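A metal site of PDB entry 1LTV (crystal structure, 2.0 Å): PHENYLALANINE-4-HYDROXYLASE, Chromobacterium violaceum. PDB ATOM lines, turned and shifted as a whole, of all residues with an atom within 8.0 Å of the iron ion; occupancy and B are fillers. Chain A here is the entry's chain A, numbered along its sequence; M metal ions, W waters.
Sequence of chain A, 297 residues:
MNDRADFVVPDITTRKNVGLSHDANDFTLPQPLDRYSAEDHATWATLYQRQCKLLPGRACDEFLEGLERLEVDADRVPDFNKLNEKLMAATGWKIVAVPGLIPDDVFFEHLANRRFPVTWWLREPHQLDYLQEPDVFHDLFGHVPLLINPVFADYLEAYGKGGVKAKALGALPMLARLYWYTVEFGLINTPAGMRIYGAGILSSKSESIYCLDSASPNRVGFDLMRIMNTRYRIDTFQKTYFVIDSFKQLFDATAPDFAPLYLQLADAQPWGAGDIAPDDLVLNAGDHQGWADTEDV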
ATOM      1  N   PHE A 107     -16.881  22.037 -14.242  1.00  0.00           N
ATOM      2  CA  PHE A 107     -17.601  21.291 -13.220  1.00  0.00           C
ATOM      3  C   PHE A 107     -18.173  19.983 -13.797  1.00  0.00           C
ATOM      4  O   PHE A 107     -18.015  18.935 -13.204  1.00  0.00           O
ATOM      5  CB  PHE A 107     -18.719  22.160 -12.658  1.00  0.00           C
ATOM      6  CG  PHE A 107     -19.526  21.491 -11.584  1.00  0.00           C
ATOM      7  CD1 PHE A 107     -19.124  21.542 -10.258  1.00  0.00           C
ATOM      8  CD2 PHE A 107     -20.737  20.889 -11.894  1.00  0.00           C
ATOM      9  CE1 PHE A 107     -19.910  21.010  -9.238  1.00  0.00           C
ATOM     10  CE2 PHE A 107     -21.551  20.345 -10.867  1.00  0.00           C
ATOM     11  CZ  PHE A 107     -21.134  20.412  -9.538  1.00  0.00           C
ATOM     12  N   PHE A 116     -15.147  15.199  -7.372  1.00  0.00           N
ATOM     13  CA  PHE A 116     -16.069  16.167  -6.872  1.00  0.00           C
ATOM     14  C   PHE A 116     -15.298  17.411  -6.422  1.00  0.00           C
ATOM     15  O   PHE A 116     -14.520  17.370  -5.465  1.00  0.00           O
ATOM     16  CB  PHE A 116     -16.894  15.635  -5.700  1.00  0.00           C
ATOM     17  CG  PHE A 116     -18.026  16.549  -5.343  1.00  0.00           C
ATOM     18  CD1 PHE A 116     -19.202  16.532  -6.106  1.00  0.00           C
ATOM     19  CD2 PHE A 116     -17.870  17.517  -4.375  1.00  0.00           C
ATOM     20  CE1 PHE A 116     -20.206  17.467  -5.892  1.00  0.00           C
ATOM     21  CE2 PHE A 116     -18.881  18.469  -4.158  1.00  0.00           C
ATOM     22  CZ  PHE A 116     -20.032  18.439  -4.912  1.00  0.00           C
ATOM     23  N   PRO A 117     -15.538  18.559  -7.079  1.00  0.00           N
ATOM     24  CA  PRO A 117     -14.811  19.765  -6.690  1.00  0.00           C
ATOM     25  C   PRO A 117     -15.273  20.275  -5.342  1.00  0.00           C
ATOM     26  O   PRO A 117     -16.463  20.352  -5.106  1.00  0.00           O
ATOM     27  CB  PRO A 117     -15.169  20.766  -7.791  1.00  0.00           C
ATOM     28  CG  PRO A 117     -15.706  19.948  -8.890  1.00  0.00           C
ATOM     29  CD  PRO A 117     -16.465  18.852  -8.176  1.00  0.00           C
ATOM     30  N   TYR A 130     -25.196  28.953   5.611  1.00  0.00           N
ATOM     31  CA  TYR A 130     -25.248  29.019   4.141  1.00  0.00           C
ATOM     32  C   TYR A 130     -25.082  30.452   3.611  1.00  0.00           C
ATOM     33  O   TYR A 130     -26.008  31.021   3.019  1.00  0.00           O
ATOM     34  CB  TYR A 130     -26.569  28.404   3.619  1.00  0.00           C
ATOM     35  CG  TYR A 130     -26.462  27.731   2.242  1.00  0.00           C
ATOM     36  CD1 TYR A 130     -26.362  26.335   2.128  1.00  0.00           C
ATOM     37  CD2 TYR A 130     -26.417  28.497   1.071  1.00  0.00           C
ATOM     38  CE1 TYR A 130     -26.202  25.715   0.867  1.00  0.00           C
ATOM     39  CE2 TYR A 130     -26.256  27.879  -0.200  1.00  0.00           C
ATOM     40  CZ  TYR A 130     -26.151  26.491  -0.291  1.00  0.00           C
ATOM     41  OH  TYR A 130     -25.991  25.888  -1.519  1.00  0.00           O
ATOM     42  N   PRO A 134     -20.445  28.892  -1.585  1.00  0.00           N
ATOM     43  CA  PRO A 134     -20.264  27.640  -0.839  1.00  0.00           C
ATOM     44  C   PRO A 134     -18.833  27.591  -0.313  1.00  0.00           C
ATOM     45  O   PRO A 134     -17.926  28.174  -0.889  1.00  0.00           O
ATOM     46  CB  PRO A 134     -20.492  26.573  -1.892  1.00  0.00           C
ATOM     47  CG  PRO A 134     -21.428  27.223  -2.826  1.00  0.00           C
ATOM     48  CD  PRO A 134     -20.879  28.620  -2.957  1.00  0.00           C
ATOM     49  N   ASP A 135     -18.622  26.882   0.789  1.00  0.00           N
ATOM     50  CA  ASP A 135     -17.289  26.767   1.349  1.00  0.00           C
ATOM     51  C   ASP A 135     -16.953  25.305   1.610  1.00  0.00           C
ATOM     52  O   ASP A 135     -17.702  24.430   1.205  1.00  0.00           O
ATOM     53  CB  ASP A 135     -17.159  27.577   2.652  1.00  0.00           C
ATOM     54  CG  ASP A 135     -17.964  27.007   3.776  1.00  0.00           C
ATOM     55  OD1 ASP A 135     -17.690  27.414   4.912  1.00  0.00           O
ATOM     56  OD2 ASP A 135     -18.873  26.189   3.558  1.00  0.00           O
ATOM     57  N   HIS A 138     -19.785  23.307   3.507  1.00  0.00           N
ATOM     58  CA  HIS A 138     -20.923  23.006   2.658  1.00  0.00           C
ATOM     59  C   HIS A 138     -20.550  21.973   1.670  1.00  0.00           C
ATOM     60  O   HIS A 138     -21.223  20.947   1.534  1.00  0.00           O
ATOM     61  CB  HIS A 138     -21.417  24.226   1.850  1.00  0.00           C
ATOM     62  CG  HIS A 138     -22.293  23.831   0.698  1.00  0.00           C
ATOM     63  ND1 HIS A 138     -23.543  23.264   0.883  1.00  0.00           N
ATOM     64  CD2 HIS A 138     -22.068  23.825  -0.630  1.00  0.00           C
ATOM     65  CE1 HIS A 138     -24.039  22.921  -0.291  1.00  0.00           C
ATOM     66  NE2 HIS A 138     -23.167  23.243  -1.228  1.00  0.00           N
ATOM     67  N   ASP A 139     -19.450  22.207   0.972  1.00  0.00           N
ATOM     68  CA  ASP A 139     -19.046  21.281  -0.065  1.00  0.00           C
ATOM     69  C   ASP A 139     -18.625  19.936   0.388  1.00  0.00           C
ATOM     70  O   ASP A 139     -18.903  18.945  -0.295  1.00  0.00           O
ATOM     71  CB  ASP A 139     -17.900  21.855  -0.917  1.00  0.00           C
ATOM     72  CG  ASP A 139     -18.388  22.824  -2.000  1.00  0.00           C
ATOM     73  OD1 ASP A 139     -19.616  22.934  -2.259  1.00  0.00           O
ATOM     74  OD2 ASP A 139     -17.521  23.495  -2.601  1.00  0.00           O
ATOM     75  N   LEU A 140     -17.918  19.859   1.508  1.00  0.00           N
ATOM     76  CA  LEU A 140     -17.434  18.585   1.937  1.00  0.00           C
ATOM     77  C   LEU A 140     -18.440  17.870   2.849  1.00  0.00           C
ATOM     78  O   LEU A 140     -18.782  16.713   2.579  1.00  0.00           O
ATOM     79  CB  LEU A 140     -16.039  18.769   2.601  1.00  0.00           C
ATOM     80  CG  LEU A 140     -15.191  17.484   2.789  1.00  0.00           C
ATOM     81  CD1 LEU A 140     -13.770  17.851   3.215  1.00  0.00           C
ATOM     82  CD2 LEU A 140     -15.829  16.599   3.908  1.00  0.00           C
ATOM     83  N   GLY A 142     -21.698  18.601   3.377  1.00  0.00           N
ATOM     84  CA  GLY A 142     -22.974  18.437   2.734  1.00  0.00           C
ATOM     85  C   GLY A 142     -23.018  17.573   1.495  1.00  0.00           C
ATOM     86  O   GLY A 142     -23.984  16.896   1.334  1.00  0.00           O
ATOM     87  N   HIS A 143     -21.983  17.593   0.648  1.00  0.00           N
ATOM     88  CA  HIS A 143     -21.952  16.823  -0.598  1.00  0.00           C
ATOM     89  C   HIS A 143     -21.300  15.447  -0.560  1.00  0.00           C
ATOM     90  O   HIS A 143     -21.843  14.490  -1.095  1.00  0.00           O
ATOM     91  CB  HIS A 143     -21.236  17.605  -1.704  1.00  0.00           C
ATOM     92  CG  HIS A 143     -22.067  18.666  -2.346  1.00  0.00           C
ATOM     93  ND1 HIS A 143     -23.032  18.398  -3.312  1.00  0.00           N
ATOM     94  CD2 HIS A 143     -22.113  20.001  -2.140  1.00  0.00           C
ATOM     95  CE1 HIS A 143     -23.623  19.529  -3.663  1.00  0.00           C
ATOM     96  NE2 HIS A 143     -23.085  20.509  -2.970  1.00  0.00           N
ATOM     97  N   TYR A 179     -29.764  20.164 -10.967  1.00  0.00           N
ATOM     98  CA  TYR A 179     -28.756  19.938  -9.945  1.00  0.00           C
ATOM     99  C   TYR A 179     -29.230  20.543  -8.609  1.00  0.00           C
ATOM    100  O   TYR A 179     -29.129  19.940  -7.542  1.00  0.00           O
ATOM    101  CB  TYR A 179     -27.448  20.606 -10.383  1.00  0.00           C
ATOM    102  CG  TYR A 179     -26.257  20.299  -9.481  1.00  0.00           C
ATOM    103  CD1 TYR A 179     -25.543  19.110  -9.626  1.00  0.00           C
ATOM    104  CD2 TYR A 179     -25.869  21.208  -8.483  1.00  0.00           C
ATOM    105  CE1 TYR A 179     -24.447  18.821  -8.787  1.00  0.00           C
ATOM    106  CE2 TYR A 179     -24.799  20.935  -7.661  1.00  0.00           C
ATOM    107  CZ  TYR A 179     -24.090  19.736  -7.820  1.00  0.00           C
ATOM    108  OH  TYR A 179     -23.017  19.449  -6.980  1.00  0.00           O
ATOM    109  N   TRP A 180     -29.722  21.764  -8.712  1.00  0.00           N
ATOM    110  CA  TRP A 180     -30.194  22.511  -7.552  1.00  0.00           C
ATOM    111  C   TRP A 180     -31.325  21.810  -6.806  1.00  0.00           C
ATOM    112  O   TRP A 180     -31.354  21.811  -5.572  1.00  0.00           O
ATOM    113  CB  TRP A 180     -30.663  23.872  -8.014  1.00  0.00           C
ATOM    114  CG  TRP A 180     -31.139  24.768  -6.905  1.00  0.00           C
ATOM    115  CD1 TRP A 180     -32.420  24.892  -6.408  1.00  0.00           C
ATOM    116  CD2 TRP A 180     -30.335  25.683  -6.193  1.00  0.00           C
ATOM    117  NE1 TRP A 180     -32.445  25.854  -5.429  1.00  0.00           N
ATOM    118  CE2 TRP A 180     -31.168  26.358  -5.278  1.00  0.00           C
ATOM    119  CE3 TRP A 180     -28.974  26.017  -6.236  1.00  0.00           C
ATOM    120  CZ2 TRP A 180     -30.684  27.345  -4.434  1.00  0.00           C
ATOM    121  CZ3 TRP A 180     -28.498  27.000  -5.393  1.00  0.00           C
ATOM    122  CH2 TRP A 180     -29.355  27.659  -4.503  1.00  0.00           C
ATOM    123  N   VAL A 183     -29.389  17.441  -6.138  1.00  0.00           N
ATOM    124  CA  VAL A 183     -28.141  17.461  -5.361  1.00  0.00           C
ATOM    125  C   VAL A 183     -28.040  18.495  -4.219  1.00  0.00           C
ATOM    126  O   VAL A 183     -27.524  18.187  -3.124  1.00  0.00           O
ATOM    127  CB  VAL A 183     -26.922  17.656  -6.307  1.00  0.00           C
ATOM    128  CG1 VAL A 183     -25.612  17.500  -5.512  1.00  0.00           C
ATOM    129  CG2 VAL A 183     -27.021  16.640  -7.426  1.00  0.00           C
ATOM    130  N   GLU A 184     -28.534  19.712  -4.476  1.00  0.00           N
ATOM    131  CA  GLU A 184     -28.520  20.755  -3.448  1.00  0.00           C
ATOM    132  C   GLU A 184     -29.749  20.794  -2.496  1.00  0.00           C
ATOM    133  O   GLU A 184     -29.600  20.933  -1.287  1.00  0.00           O
ATOM    134  CB  GLU A 184     -28.378  22.145  -4.090  1.00  0.00           C
ATOM    135  CG  GLU A 184     -27.183  22.284  -5.018  1.00  0.00           C
ATOM    136  CD  GLU A 184     -25.894  22.429  -4.245  1.00  0.00           C
ATOM    137  OE1 GLU A 184     -25.895  22.286  -2.997  1.00  0.00           O
ATOM    138  OE2 GLU A 184     -24.864  22.727  -4.903  1.00  0.00           O
ATOM    139  N   PHE A 185     -30.955  20.673  -3.046  1.00  0.00           N
ATOM    140  CA  PHE A 185     -32.131  20.805  -2.196  1.00  0.00           C
ATOM    141  C   PHE A 185     -33.136  19.678  -2.296  1.00  0.00           C
ATOM    142  O   PHE A 185     -34.308  19.879  -2.044  1.00  0.00           O
ATOM    143  CB  PHE A 185     -32.830  22.153  -2.477  1.00  0.00           C
ATOM    144  CG  PHE A 185     -32.028  23.327  -1.988  1.00  0.00           C
ATOM    145  CD1 PHE A 185     -31.043  23.921  -2.813  1.00  0.00           C
ATOM    146  CD2 PHE A 185     -32.103  23.712  -0.637  1.00  0.00           C
ATOM    147  CE1 PHE A 185     -30.151  24.843  -2.310  1.00  0.00           C
ATOM    148  CE2 PHE A 185     -31.202  24.655  -0.109  1.00  0.00           C
ATOM    149  CZ  PHE A 185     -30.210  25.213  -0.962  1.00  0.00           C
ATOM    150  N   GLY A 198     -30.328  16.591   0.009  1.00  0.00           N
ATOM    151  CA  GLY A 198     -29.701  17.774  -0.571  1.00  0.00           C
ATOM    152  C   GLY A 198     -28.586  18.403   0.282  1.00  0.00           C
ATOM    153  O   GLY A 198     -28.753  18.651   1.478  1.00  0.00           O
ATOM    154  N   ALA A 199     -27.451  18.672  -0.357  1.00  0.00           N
ATOM    155  CA  ALA A 199     -26.279  19.239   0.302  1.00  0.00           C
ATOM    156  C   ALA A 199     -26.494  20.629   0.858  1.00  0.00           C
ATOM    157  O   ALA A 199     -25.954  20.943   1.927  1.00  0.00           O
ATOM    158  CB  ALA A 199     -25.101  19.264  -0.690  1.00  0.00           C
ATOM    159  N   GLY A 200     -27.230  21.466   0.095  1.00  0.00           N
ATOM    160  CA  GLY A 200     -27.504  22.824   0.530  1.00  0.00           C
ATOM    161  C   GLY A 200     -28.380  22.859   1.762  1.00  0.00           C
ATOM    162  O   GLY A 200     -28.447  23.837   2.508  1.00  0.00           O
ATOM    163  N   ILE A 201     -29.095  21.772   1.990  1.00  0.00           N
ATOM    164  CA  ILE A 201     -29.955  21.660   3.173  1.00  0.00           C
ATOM    165  C   ILE A 201     -29.165  21.041   4.341  1.00  0.00           C
ATOM    166  O   ILE A 201     -29.232  21.534   5.479  1.00  0.00           O
ATOM    167  CB  ILE A 201     -31.176  20.702   2.944  1.00  0.00           C
ATOM    168  CG1 ILE A 201     -32.140  21.285   1.904  1.00  0.00           C
ATOM    169  CG2 ILE A 201     -31.889  20.486   4.287  1.00  0.00           C
ATOM    170  CD1 ILE A 201     -33.235  20.272   1.414  1.00  0.00           C
ATOM    171  N   SER A 203     -25.985  20.926   5.027  1.00  0.00           N
ATOM    172  CA  SER A 203     -24.913  21.685   5.669  1.00  0.00           C
ATOM    173  C   SER A 203     -25.515  22.932   6.321  1.00  0.00           C
ATOM    174  O   SER A 203     -24.792  23.710   6.961  1.00  0.00           O
ATOM    175  CB  SER A 203     -23.838  22.068   4.642  1.00  0.00           C
ATOM    176  OG  SER A 203     -24.310  23.007   3.696  1.00  0.00           O
HETATM  177 FE    FE M   1     -23.509  22.819  -3.177  1.00  0.00          FE
HETATM  178  O   HOH W   1     -21.690  23.227  -3.971  1.00  0.00           O
HETATM  179  O   HOH W   2     -24.325  25.060  -3.294  1.00  0.00           O
HETATM  180  O   HOH W   3     -21.552  21.747  -5.856  1.00  0.00           O
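Three residues have an atom within 4 Å of the iron ion: His 138, His 143 and Glu 184.
The nearest printed residue that does not touch the iron ion is Asp 139 (4.001 Å).
The backbone NH of Glu 184 is in hydrogen-bond range of the backbone carbonyl oxygen of Tyr 179.
O of Glu 184 sits at hydrogen-bond distance from N of Gly 200.
The backbone NH (N) of Ala 199 lies within hydrogen-bond range of the backbone carbonyl oxygen (O) of Glu 184, 3.3 Å away.
O of Glu 184 sits at hydrogen-bond distance from N of Ile 201, at 3.4 Å.
A ring nitrogen (ND1) of His 138 sits at hydrogen-bond distance from the side-chain hydroxyl (OG) of Ser 203 (2.9 Å).
OD2 of Asp 135 is in hydrogen-bond range of N of His 138.
The iron ion is bound by a ring nitrogen (NE2) of His 138 (2.0 Å), water W1 (2.0 Å), the side-chain carboxylate (OE2) of Glu 184 (2.2 Å), a ring nitrogen (NE2) of His 143 (2.4 Å), water W2 (2.4 Å) and the side-chain carboxylate (OE1) of Glu 184 (2.5 Å).
The iron ion has six donor atoms within binding distance.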
